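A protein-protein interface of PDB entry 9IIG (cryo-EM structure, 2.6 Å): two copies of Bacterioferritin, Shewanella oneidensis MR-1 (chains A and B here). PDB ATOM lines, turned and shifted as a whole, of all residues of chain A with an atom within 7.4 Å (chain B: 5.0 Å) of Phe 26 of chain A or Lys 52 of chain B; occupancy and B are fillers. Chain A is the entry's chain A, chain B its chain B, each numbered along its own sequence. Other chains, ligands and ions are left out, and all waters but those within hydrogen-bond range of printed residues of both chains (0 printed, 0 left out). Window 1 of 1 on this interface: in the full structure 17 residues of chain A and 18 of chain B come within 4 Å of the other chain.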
ATOM      1  N   LEU A  19      -6.267  16.312  27.516  1.00  0.00           N
ATOM      2  CA  LEU A  19      -5.776  17.273  28.494  1.00  0.00           C
ATOM      3  C   LEU A  19      -4.305  17.586  28.261  1.00  0.00           C
ATOM      4  O   LEU A  19      -3.879  18.744  28.368  1.00  0.00           O
ATOM      5  CB  LEU A  19      -6.005  16.728  29.899  1.00  0.00           C
ATOM      6  CG  LEU A  19      -7.466  16.727  30.342  1.00  0.00           C
ATOM      7  CD1 LEU A  19      -7.623  15.994  31.645  1.00  0.00           C
ATOM      8  CD2 LEU A  19      -8.010  18.123  30.447  1.00  0.00           C
ATOM      9  N   SER A  20      -3.513  16.567  27.920  1.00  0.00           N
ATOM     10  CA  SER A  20      -2.123  16.807  27.555  1.00  0.00           C
ATOM     11  C   SER A  20      -2.021  17.654  26.294  1.00  0.00           C
ATOM     12  O   SER A  20      -1.152  18.529  26.195  1.00  0.00           O
ATOM     13  CB  SER A  20      -1.398  15.482  27.371  1.00  0.00           C
ATOM     14  OG  SER A  20      -1.348  14.765  28.586  1.00  0.00           O
ATOM     15  N   ALA A  21      -2.889  17.399  25.312  1.00  0.00           N
ATOM     16  CA  ALA A  21      -2.946  18.238  24.122  1.00  0.00           C
ATOM     17  C   ALA A  21      -3.234  19.680  24.481  1.00  0.00           C
ATOM     18  O   ALA A  21      -2.633  20.600  23.922  1.00  0.00           O
ATOM     19  CB  ALA A  21      -4.016  17.726  23.163  1.00  0.00           C
ATOM     20  N   MET A  22      -4.187  19.896  25.381  1.00  0.00           N
ATOM     21  CA  MET A  22      -4.506  21.242  25.831  1.00  0.00           C
ATOM     22  C   MET A  22      -3.286  21.937  26.415  1.00  0.00           C
ATOM     23  O   MET A  22      -2.988  23.081  26.064  1.00  0.00           O
ATOM     24  CB  MET A  22      -5.624  21.184  26.860  1.00  0.00           C
ATOM     25  CG  MET A  22      -6.048  22.522  27.370  1.00  0.00           C
ATOM     26  SD  MET A  22      -7.357  22.311  28.566  1.00  0.00           S
ATOM     27  CE  MET A  22      -6.446  21.602  29.934  1.00  0.00           C
ATOM     28  N   ASP A  23      -2.572  21.261  27.315  1.00  0.00           N
ATOM     29  CA  ASP A  23      -1.387  21.872  27.916  1.00  0.00           C
ATOM     30  C   ASP A  23      -0.329  22.198  26.872  1.00  0.00           C
ATOM     31  O   ASP A  23       0.266  23.284  26.892  1.00  0.00           O
ATOM     32  CB  ASP A  23      -0.805  20.955  28.983  1.00  0.00           C
ATOM     33  CG  ASP A  23      -1.609  20.958  30.243  1.00  0.00           C
ATOM     34  OD1 ASP A  23      -2.299  21.962  30.507  1.00  0.00           O
ATOM     35  OD2 ASP A  23      -1.545  19.954  30.978  1.00  0.00           O
ATOM     36  N   GLN A  24      -0.065  21.261  25.962  1.00  0.00           N
ATOM     37  CA  GLN A  24       0.981  21.475  24.968  1.00  0.00           C
ATOM     38  C   GLN A  24       0.619  22.608  24.019  1.00  0.00           C
ATOM     39  O   GLN A  24       1.455  23.460  23.714  1.00  0.00           O
ATOM     40  CB  GLN A  24       1.246  20.185  24.200  1.00  0.00           C
ATOM     41  CG  GLN A  24       2.510  20.231  23.384  1.00  0.00           C
ATOM     42  CD  GLN A  24       2.779  18.954  22.640  1.00  0.00           C
ATOM     43  OE1 GLN A  24       3.018  17.910  23.238  1.00  0.00           O
ATOM     44  NE2 GLN A  24       2.732  19.024  21.322  1.00  0.00           N
ATOM     45  N   TYR A  25      -0.629  22.647  23.557  1.00  0.00           N
ATOM     46  CA  TYR A  25      -1.063  23.722  22.674  1.00  0.00           C
ATOM     47  C   TYR A  25      -1.054  25.055  23.399  1.00  0.00           C
ATOM     48  O   TYR A  25      -0.770  26.090  22.799  1.00  0.00           O
ATOM     49  CB  TYR A  25      -2.460  23.424  22.143  1.00  0.00           C
ATOM     50  CG  TYR A  25      -2.513  22.250  21.214  1.00  0.00           C
ATOM     51  CD1 TYR A  25      -1.365  21.751  20.640  1.00  0.00           C
ATOM     52  CD2 TYR A  25      -3.705  21.612  20.943  1.00  0.00           C
ATOM     53  CE1 TYR A  25      -1.403  20.670  19.810  1.00  0.00           C
ATOM     54  CE2 TYR A  25      -3.752  20.532  20.112  1.00  0.00           C
ATOM     55  CZ  TYR A  25      -2.597  20.066  19.548  1.00  0.00           C
ATOM     56  OH  TYR A  25      -2.625  18.986  18.716  1.00  0.00           O
ATOM     57  N   PHE A  26      -1.340  25.042  24.696  1.00  0.00           N
ATOM     58  CA  PHE A  26      -1.328  26.260  25.495  1.00  0.00           C
ATOM     59  C   PHE A  26       0.079  26.844  25.575  1.00  0.00           C
ATOM     60  O   PHE A  26       0.306  28.015  25.233  1.00  0.00           O
ATOM     61  CB  PHE A  26      -1.900  25.903  26.869  1.00  0.00           C
ATOM     62  CG  PHE A  26      -1.803  26.973  27.902  1.00  0.00           C
ATOM     63  CD1 PHE A  26      -2.578  28.113  27.818  1.00  0.00           C
ATOM     64  CD2 PHE A  26      -0.997  26.797  29.012  1.00  0.00           C
ATOM     65  CE1 PHE A  26      -2.505  29.079  28.796  1.00  0.00           C
ATOM     66  CE2 PHE A  26      -0.923  27.757  29.988  1.00  0.00           C
ATOM     67  CZ  PHE A  26      -1.675  28.899  29.880  1.00  0.00           C
ATOM     68  N   VAL A  27       1.052  26.023  25.975  1.00  0.00           N
ATOM     69  CA  VAL A  27       2.410  26.538  26.107  1.00  0.00           C
ATOM     70  C   VAL A  27       2.992  26.881  24.740  1.00  0.00           C
ATOM     71  O   VAL A  27       3.745  27.844  24.608  1.00  0.00           O
ATOM     72  CB  VAL A  27       3.300  25.553  26.889  1.00  0.00           C
ATOM     73  CG1 VAL A  27       3.342  24.217  26.220  1.00  0.00           C
ATOM     74  CG2 VAL A  27       4.697  26.106  27.073  1.00  0.00           C
ATOM     75  N   HIS A  28       2.622  26.136  23.693  1.00  0.00           N
ATOM     76  CA  HIS A  28       3.119  26.459  22.359  1.00  0.00           C
ATOM     77  C   HIS A  28       2.527  27.754  21.829  1.00  0.00           C
ATOM     78  O   HIS A  28       3.235  28.551  21.213  1.00  0.00           O
ATOM     79  CB  HIS A  28       2.838  25.318  21.387  1.00  0.00           C
ATOM     80  CG  HIS A  28       3.822  24.197  21.472  1.00  0.00           C
ATOM     81  ND1 HIS A  28       3.683  23.030  20.755  1.00  0.00           N
ATOM     82  CD2 HIS A  28       4.977  24.076  22.163  1.00  0.00           C
ATOM     83  CE1 HIS A  28       4.700  22.231  21.017  1.00  0.00           C
ATOM     84  NE2 HIS A  28       5.501  22.842  21.867  1.00  0.00           N
ATOM     85  N   ALA A  29       1.231  27.979  22.036  1.00  0.00           N
ATOM     86  CA  ALA A  29       0.638  29.242  21.629  1.00  0.00           C
ATOM     87  C   ALA A  29       1.321  30.401  22.324  1.00  0.00           C
ATOM     88  O   ALA A  29       1.598  31.435  21.708  1.00  0.00           O
ATOM     89  CB  ALA A  29      -0.856  29.245  21.931  1.00  0.00           C
ATOM     90  N   HIS A  30       1.637  30.241  23.605  1.00  0.00           N
ATOM     91  CA  HIS A  30       2.255  31.358  24.302  1.00  0.00           C
ATOM     92  C   HIS A  30       3.719  31.525  23.923  1.00  0.00           C
ATOM     93  O   HIS A  30       4.235  32.644  23.948  1.00  0.00           O
ATOM     94  CB  HIS A  30       2.069  31.185  25.798  1.00  0.00           C
ATOM     95  CG  HIS A  30       0.675  31.474  26.247  1.00  0.00           C
ATOM     96  ND1 HIS A  30      -0.008  32.602  25.855  1.00  0.00           N
ATOM     97  CD2 HIS A  30      -0.185  30.759  27.007  1.00  0.00           C
ATOM     98  CE1 HIS A  30      -1.219  32.584  26.378  1.00  0.00           C
ATOM     99  NE2 HIS A  30      -1.352  31.476  27.080  1.00  0.00           N
ATOM    100  N   MET A  31       4.400  30.443  23.547  1.00  0.00           N
ATOM    101  CA  MET A  31       5.751  30.577  23.015  1.00  0.00           C
ATOM    102  C   MET A  31       5.735  31.253  21.653  1.00  0.00           C
ATOM    103  O   MET A  31       6.688  31.942  21.284  1.00  0.00           O
ATOM    104  CB  MET A  31       6.420  29.211  22.921  1.00  0.00           C
ATOM    105  CG  MET A  31       6.725  28.572  24.248  1.00  0.00           C
ATOM    106  SD  MET A  31       7.208  26.857  24.072  1.00  0.00           S
ATOM    107  CE  MET A  31       8.699  27.062  23.120  1.00  0.00           C
ATOM    108  N   TYR A  32       4.663  31.059  20.886  1.00  0.00           N
ATOM    109  CA  TYR A  32       4.523  31.755  19.613  1.00  0.00           C
ATOM    110  C   TYR A  32       4.254  33.232  19.832  1.00  0.00           C
ATOM    111  O   TYR A  32       4.764  34.079  19.096  1.00  0.00           O
ATOM    112  CB  TYR A  32       3.394  31.135  18.794  1.00  0.00           C
ATOM    113  CG  TYR A  32       3.754  29.824  18.156  1.00  0.00           C
ATOM    114  CD1 TYR A  32       4.995  29.629  17.588  1.00  0.00           C
ATOM    115  CD2 TYR A  32       2.857  28.773  18.145  1.00  0.00           C
ATOM    116  CE1 TYR A  32       5.326  28.433  17.020  1.00  0.00           C
ATOM    117  CE2 TYR A  32       3.181  27.576  17.584  1.00  0.00           C
ATOM    118  CZ  TYR A  32       4.414  27.411  17.022  1.00  0.00           C
ATOM    119  OH  TYR A  32       4.740  26.210  16.456  1.00  0.00           O
ATOM    120  N   TYR A  41       0.127  31.995  17.347  1.00  0.00           N
ATOM    121  CA  TYR A  41      -0.390  32.064  18.707  1.00  0.00           C
ATOM    122  C   TYR A  41      -1.897  31.885  18.713  1.00  0.00           C
ATOM    123  O   TYR A  41      -2.435  31.081  19.477  1.00  0.00           O
ATOM    124  CB  TYR A  41      -0.032  33.391  19.366  1.00  0.00           C
ATOM    125  CG  TYR A  41      -0.941  33.717  20.531  1.00  0.00           C
ATOM    126  CD1 TYR A  41      -0.909  32.954  21.687  1.00  0.00           C
ATOM    127  CD2 TYR A  41      -1.851  34.757  20.469  1.00  0.00           C
ATOM    128  CE1 TYR A  41      -1.732  33.221  22.755  1.00  0.00           C
ATOM    129  CE2 TYR A  41      -2.688  35.031  21.537  1.00  0.00           C
ATOM    130  CZ  TYR A  41      -2.620  34.255  22.679  1.00  0.00           C
ATOM    131  OH  TYR A  41      -3.436  34.500  23.756  1.00  0.00           O
ATOM    132  N   ILE A  44      -3.008  28.228  17.553  1.00  0.00           N
ATOM    133  CA  ILE A  44      -2.721  27.183  18.526  1.00  0.00           C
ATOM    134  C   ILE A  44      -3.521  27.396  19.803  1.00  0.00           C
ATOM    135  O   ILE A  44      -3.891  26.429  20.479  1.00  0.00           O
ATOM    136  CB  ILE A  44      -1.209  27.124  18.788  1.00  0.00           C
ATOM    137  CG1 ILE A  44      -0.456  26.874  17.490  1.00  0.00           C
ATOM    138  CG2 ILE A  44      -0.870  26.001  19.707  1.00  0.00           C
ATOM    139  CD1 ILE A  44      -0.807  25.582  16.823  1.00  0.00           C
ATOM    140  N   ALA A  45      -3.842  28.644  20.145  1.00  0.00           N
ATOM    141  CA  ALA A  45      -4.693  28.885  21.304  1.00  0.00           C
ATOM    142  C   ALA A  45      -6.116  28.421  21.040  1.00  0.00           C
ATOM    143  O   ALA A  45      -6.759  27.834  21.918  1.00  0.00           O
ATOM    144  CB  ALA A  45      -4.673  30.364  21.678  1.00  0.00           C
ATOM    145  N   GLU A  47      -6.842  26.015  19.129  1.00  0.00           N
ATOM    146  CA  GLU A  47      -6.795  24.558  19.175  1.00  0.00           C
ATOM    147  C   GLU A  47      -6.736  24.041  20.603  1.00  0.00           C
ATOM    148  O   GLU A  47      -7.293  22.983  20.905  1.00  0.00           O
ATOM    149  CB  GLU A  47      -5.627  24.032  18.355  1.00  0.00           C
ATOM    150  CG  GLU A  47      -5.850  24.316  16.911  1.00  0.00           C
ATOM    151  CD  GLU A  47      -7.042  23.545  16.383  1.00  0.00           C
ATOM    152  OE1 GLU A  47      -7.297  22.427  16.883  1.00  0.00           O
ATOM    153  OE2 GLU A  47      -7.742  24.069  15.494  1.00  0.00           O
ATOM    154  N   SER A  48      -6.081  24.771  21.499  1.00  0.00           N
ATOM    155  CA  SER A  48      -6.144  24.404  22.908  1.00  0.00           C
ATOM    156  C   SER A  48      -7.570  24.523  23.436  1.00  0.00           C
ATOM    157  O   SER A  48      -8.021  23.697  24.238  1.00  0.00           O
ATOM    158  CB  SER A  48      -5.186  25.272  23.715  1.00  0.00           C
ATOM    159  OG  SER A  48      -5.254  24.952  25.088  1.00  0.00           O
ATOM    160  N   ASP A  49      -8.309  25.532  22.975  1.00  0.00           N
ATOM    161  CA  ASP A  49      -9.712  25.652  23.368  1.00  0.00           C
ATOM    162  C   ASP A  49     -10.548  24.499  22.825  1.00  0.00           C
ATOM    163  O   ASP A  49     -11.447  23.998  23.510  1.00  0.00           O
ATOM    164  CB  ASP A  49     -10.285  26.988  22.906  1.00  0.00           C
ATOM    165  CG  ASP A  49      -9.695  28.158  23.651  1.00  0.00           C
ATOM    166  OD1 ASP A  49      -9.304  27.976  24.819  1.00  0.00           O
ATOM    167  OD2 ASP A  49      -9.640  29.263  23.077  1.00  0.00           O
ATOM    168  N   LYS A  52     -10.009  21.641  24.973  1.00  0.00           N
ATOM    169  CA  LYS A  52     -10.810  21.782  26.188  1.00  0.00           C
ATOM    170  C   LYS A  52     -12.259  21.378  25.943  1.00  0.00           C
ATOM    171  O   LYS A  52     -12.890  20.754  26.799  1.00  0.00           O
ATOM    172  CB  LYS A  52     -10.721  23.217  26.713  1.00  0.00           C
ATOM    173  CG  LYS A  52     -11.112  23.411  28.186  1.00  0.00           C
ATOM    174  CD  LYS A  52     -10.687  22.250  29.074  1.00  0.00           C
ATOM    175  CE  LYS A  52     -10.446  22.705  30.502  1.00  0.00           C
ATOM    176  NZ  LYS A  52      -9.876  21.626  31.356  1.00  0.00           N
ATOM    177  N   LEU A  77       4.587  15.910  28.017  1.00  0.00           N
ATOM    178  CA  LEU A  77       4.487  16.944  27.003  1.00  0.00           C
ATOM    179  C   LEU A  77       5.781  16.995  26.213  1.00  0.00           C
ATOM    180  O   LEU A  77       6.866  16.830  26.776  1.00  0.00           O
ATOM    181  CB  LEU A  77       4.198  18.307  27.630  1.00  0.00           C
ATOM    182  CG  LEU A  77       2.776  18.640  28.071  1.00  0.00           C
ATOM    183  CD1 LEU A  77       2.365  17.871  29.297  1.00  0.00           C
ATOM    184  CD2 LEU A  77       2.698  20.108  28.346  1.00  0.00           C
ATOM    185  N   ASP A  90       3.386  18.968  17.701  1.00  0.00           N
ATOM    186  CA  ASP A  90       1.933  18.990  17.626  1.00  0.00           C
ATOM    187  C   ASP A  90       1.422  17.959  16.632  1.00  0.00           C
ATOM    188  O   ASP A  90       0.401  17.309  16.873  1.00  0.00           O
ATOM    189  CB  ASP A  90       1.439  20.383  17.253  1.00  0.00           C
ATOM    190  CG  ASP A  90       1.680  21.401  18.345  1.00  0.00           C
ATOM    191  OD1 ASP A  90       1.668  21.022  19.531  1.00  0.00           O
ATOM    192  OD2 ASP A  90       1.857  22.595  18.021  1.00  0.00           O
ATOM    193  N   LEU B  15       1.814  29.152  38.626  1.00  0.00           N
ATOM    194  CA  LEU B  15       1.248  28.565  37.419  1.00  0.00           C
ATOM    195  C   LEU B  15       0.759  27.146  37.668  1.00  0.00           C
ATOM    196  O   LEU B  15      -0.325  26.768  37.215  1.00  0.00           O
ATOM    197  CB  LEU B  15       2.289  28.580  36.306  1.00  0.00           C
ATOM    198  CG  LEU B  15       1.853  28.003  34.970  1.00  0.00           C
ATOM    199  CD1 LEU B  15       0.650  28.755  34.449  1.00  0.00           C
ATOM    200  CD2 LEU B  15       3.004  28.054  34.008  1.00  0.00           C
ATOM    201  N   LEU B  19      -3.136  25.956  37.243  1.00  0.00           N
ATOM    202  CA  LEU B  19      -3.500  24.859  36.357  1.00  0.00           C
ATOM    203  C   LEU B  19      -4.232  23.763  37.119  1.00  0.00           C
ATOM    204  O   LEU B  19      -5.211  23.191  36.619  1.00  0.00           O
ATOM    205  CB  LEU B  19      -2.246  24.315  35.681  1.00  0.00           C
ATOM    206  CG  LEU B  19      -1.656  25.237  34.617  1.00  0.00           C
ATOM    207  CD1 LEU B  19      -0.322  24.719  34.151  1.00  0.00           C
ATOM    208  CD2 LEU B  19      -2.595  25.412  33.459  1.00  0.00           C
ATOM    209  N   MET B  22      -7.678  24.989  37.628  1.00  0.00           N
ATOM    210  CA  MET B  22      -8.446  24.793  36.409  1.00  0.00           C
ATOM    211  C   MET B  22      -8.982  23.375  36.311  1.00  0.00           C
ATOM    212  O   MET B  22     -10.167  23.171  36.033  1.00  0.00           O
ATOM    213  CB  MET B  22      -7.573  25.111  35.203  1.00  0.00           C
ATOM    214  CG  MET B  22      -8.276  24.964  33.891  1.00  0.00           C
ATOM    215  SD  MET B  22      -7.145  25.364  32.569  1.00  0.00           S
ATOM    216  CE  MET B  22      -6.054  23.944  32.628  1.00  0.00           C
ATOM    217  N   SER B  48     -13.251  28.041  36.196  1.00  0.00           N
ATOM    218  CA  SER B  48     -12.179  27.335  35.506  1.00  0.00           C
ATOM    219  C   SER B  48     -11.647  28.164  34.339  1.00  0.00           C
ATOM    220  O   SER B  48     -10.439  28.183  34.077  1.00  0.00           O
ATOM    221  CB  SER B  48     -12.674  25.974  35.031  1.00  0.00           C
ATOM    222  OG  SER B  48     -11.659  25.287  34.334  1.00  0.00           O
ATOM    223  N   ASP B  49     -12.533  28.878  33.644  1.00  0.00           N
ATOM    224  CA  ASP B  49     -12.080  29.763  32.575  1.00  0.00           C
ATOM    225  C   ASP B  49     -11.242  30.917  33.116  1.00  0.00           C
ATOM    226  O   ASP B  49     -10.251  31.319  32.494  1.00  0.00           O
ATOM    227  CB  ASP B  49     -13.269  30.298  31.782  1.00  0.00           C
ATOM    228  CG  ASP B  49     -13.954  29.226  30.973  1.00  0.00           C
ATOM    229  OD1 ASP B  49     -13.270  28.264  30.571  1.00  0.00           O
ATOM    230  OD2 ASP B  49     -15.166  29.350  30.722  1.00  0.00           O
ATOM    231  N   ASP B  50     -11.625  31.474  34.265  1.00  0.00           N
ATOM    232  CA  ASP B  50     -10.810  32.521  34.870  1.00  0.00           C
ATOM    233  C   ASP B  50      -9.449  31.989  35.305  1.00  0.00           C
ATOM    234  O   ASP B  50      -8.442  32.692  35.201  1.00  0.00           O
ATOM    235  CB  ASP B  50     -11.532  33.160  36.050  1.00  0.00           C
ATOM    236  CG  ASP B  50     -12.921  33.613  35.698  1.00  0.00           C
ATOM    237  OD1 ASP B  50     -13.181  33.864  34.505  1.00  0.00           O
ATOM    238  OD2 ASP B  50     -13.750  33.755  36.624  1.00  0.00           O
ATOM    239  N   GLU B  51      -9.402  30.758  35.811  1.00  0.00           N
ATOM    240  CA  GLU B  51      -8.111  30.144  36.110  1.00  0.00           C
ATOM    241  C   GLU B  51      -7.272  29.987  34.852  1.00  0.00           C
ATOM    242  O   GLU B  51      -6.050  30.144  34.897  1.00  0.00           O
ATOM    243  CB  GLU B  51      -8.302  28.788  36.785  1.00  0.00           C
ATOM    244  CG  GLU B  51      -9.066  28.823  38.079  1.00  0.00           C
ATOM    245  CD  GLU B  51      -8.605  29.916  39.006  1.00  0.00           C
ATOM    246  OE1 GLU B  51      -7.531  29.759  39.617  1.00  0.00           O
ATOM    247  OE2 GLU B  51      -9.314  30.934  39.131  1.00  0.00           O
ATOM    248  N   LYS B  52      -7.905  29.660  33.725  1.00  0.00           N
ATOM    249  CA  LYS B  52      -7.172  29.587  32.463  1.00  0.00           C
ATOM    250  C   LYS B  52      -6.630  30.954  32.060  1.00  0.00           C
ATOM    251  O   LYS B  52      -5.512  31.058  31.550  1.00  0.00           O
ATOM    252  CB  LYS B  52      -8.067  29.006  31.367  1.00  0.00           C
ATOM    253  CG  LYS B  52      -7.334  28.445  30.138  1.00  0.00           C
ATOM    254  CD  LYS B  52      -6.021  27.761  30.487  1.00  0.00           C
ATOM    255  CE  LYS B  52      -5.674  26.679  29.478  1.00  0.00           C
ATOM    256  NZ  LYS B  52      -4.479  25.885  29.881  1.00  0.00           N
ATOM    257  N   GLY B  53      -7.402  32.010  32.294  1.00  0.00           N
ATOM    258  CA  GLY B  53      -6.901  33.355  32.026  1.00  0.00           C
ATOM    259  C   GLY B  53      -5.725  33.735  32.908  1.00  0.00           C
ATOM    260  O   GLY B  53      -4.749  34.331  32.442  1.00  0.00           O
ATOM    261  N   HIS B  54      -5.802  33.393  34.195  1.00  0.00           N
ATOM    262  CA  HIS B  54      -4.683  33.632  35.101  1.00  0.00           C
ATOM    263  C   HIS B  54      -3.451  32.851  34.680  1.00  0.00           C
ATOM    264  O   HIS B  54      -2.330  33.363  34.743  1.00  0.00           O
ATOM    265  CB  HIS B  54      -5.061  33.256  36.528  1.00  0.00           C
ATOM    266  CG  HIS B  54      -6.129  34.112  37.122  1.00  0.00           C
ATOM    267  ND1 HIS B  54      -6.892  33.708  38.194  1.00  0.00           N
ATOM    268  CD2 HIS B  54      -6.563  35.350  36.797  1.00  0.00           C
ATOM    269  CE1 HIS B  54      -7.748  34.663  38.505  1.00  0.00           C
ATOM    270  NE2 HIS B  54      -7.569  35.669  37.671  1.00  0.00           N
ATOM    271  N   ALA B  55      -3.637  31.600  34.266  1.00  0.00           N
ATOM    272  CA  ALA B  55      -2.507  30.796  33.821  1.00  0.00           C
ATOM    273  C   ALA B  55      -1.907  31.360  32.545  1.00  0.00           C
ATOM    274  O   ALA B  55      -0.690  31.319  32.357  1.00  0.00           O
ATOM    275  CB  ALA B  55      -2.938  29.346  33.627  1.00  0.00           C
ATOM    276  N   ALA B  56      -2.745  31.896  31.657  1.00  0.00           N
ATOM    277  CA  ALA B  56      -2.230  32.541  30.456  1.00  0.00           C
ATOM    278  C   ALA B  56      -1.385  33.751  30.808  1.00  0.00           C
ATOM    279  O   ALA B  56      -0.300  33.936  30.251  1.00  0.00           O
ATOM    280  CB  ALA B  56      -3.380  32.943  29.538  1.00  0.00           C
ATOM    281  N   VAL B  59       1.937  32.501  32.236  1.00  0.00           N
ATOM    282  CA  VAL B  59       2.807  31.949  31.203  1.00  0.00           C
ATOM    283  C   VAL B  59       3.408  33.067  30.367  1.00  0.00           C
ATOM    284  O   VAL B  59       4.602  33.047  30.049  1.00  0.00           O
ATOM    285  CB  VAL B  59       2.032  30.944  30.333  1.00  0.00           C
ATOM    286  CG1 VAL B  59       2.798  30.621  29.075  1.00  0.00           C
ATOM    287  CG2 VAL B  59       1.775  29.687  31.103  1.00  0.00           C
ATOM    288  N   VAL B  71       4.047  23.900  32.374  1.00  0.00           N
ATOM    289  CA  VAL B  71       2.650  23.501  32.292  1.00  0.00           C
ATOM    290  C   VAL B  71       2.482  21.999  32.451  1.00  0.00           C
ATOM    291  O   VAL B  71       1.353  21.501  32.365  1.00  0.00           O
ATOM    292  CB  VAL B  71       2.008  23.979  30.977  1.00  0.00           C
ATOM    293  CG1 VAL B  71       2.020  25.482  30.893  1.00  0.00           C
ATOM    294  CG2 VAL B  71       2.744  23.406  29.806  1.00  0.00           C
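The backbone carbonyl oxygen (O) of Met 22 of chain A sits at hydrogen-bond distance from the side-chain hydroxyl (OG) of Ser 48 of chain A (3.1 Å).
The side-chain hydroxyl of Ser 48 of chain B sits at hydrogen-bond distance from the backbone carbonyl oxygen of Met 22 of chain B (3.1 Å).
Met 22 of chain B touches Met 22 of chain A (CE to CE, 3.6 Å).
Asp 23 of chain A touches Val 71 of chain B.
Lys 52 of chain B touches Phe 26 of chain A (NZ to CG, 3.5 Å).
Phe 26 of chain A touches Ala 55 of chain B (CZ to O, 3.6 Å).
N of Ala 56 of chain B touches CZ of Phe 26 of chain A, at 3.6 Å.
Phe 26 of chain A touches Val 59 of chain B.
Phe 26 of chain A touches Val 71 of chain B.
Val 27 of chain A touches Val 71 of chain B.
His 30 of chain A touches Ala 56 of chain B.
Val 59 of chain B touches His 30 of chain A.
Phe 26 of chain A touches five residues of chain B.
Lys 52 of chain B touches just one residue of chain A: Phe 26 (3.5 Å).
Of the printed residues of chain B, His 30 of chain A touches Ala 56 and Val 59.
Of the printed residues of chain B, Asp 23 of chain A touches Val 71.
Printed residues of chain A within 4 Å of Ala 55 of chain B: Phe 26 (3.6 Å).
Ala 45 of chain A touches none of the printed residues of chain B.
The nearest residue of chain A that does not touch Lys 52 of chain B is Met 22 of chain A (4.5 Å).
The nearest printed residue of chain A that does not touch Ala 56 of chain B is Tyr 41 of chain A (6.0 Å).
Printed residues of chain A that touch a printed residue of chain B: Met 22, Asp 23, Phe 26, Val 27, His 30 and Leu 77.
Hydrophobic or aromatic side chains of chain A within 4 Å of the printed part of chain B: Met 22, Phe 26, Val 27, His 30 and Leu 77.
Of the 14 printed residues of chain B, 6 touch a printed residue of chain A.
Hydrophobic or aromatic side chains of chain B that line the printed part of chain A: Met 22, Ala 55, Ala 56, Val 59 and Val 71.
Among the printed residues, 11 pairs touch across the chains.
Among the printed residues, no Asp or Glu carboxylate lies within 4 Å of a Lys or Arg side-chain nitrogen of the other chain.
Met 22 of chain A touches its own counterpart, Met 22 of chain B.
Positions printed for both chains: 19, 22, 48, 49 and 52.
Of the 11 pairs that touch across the chains among the printed residues, 1 has its exchanged pair printed and touching as well.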
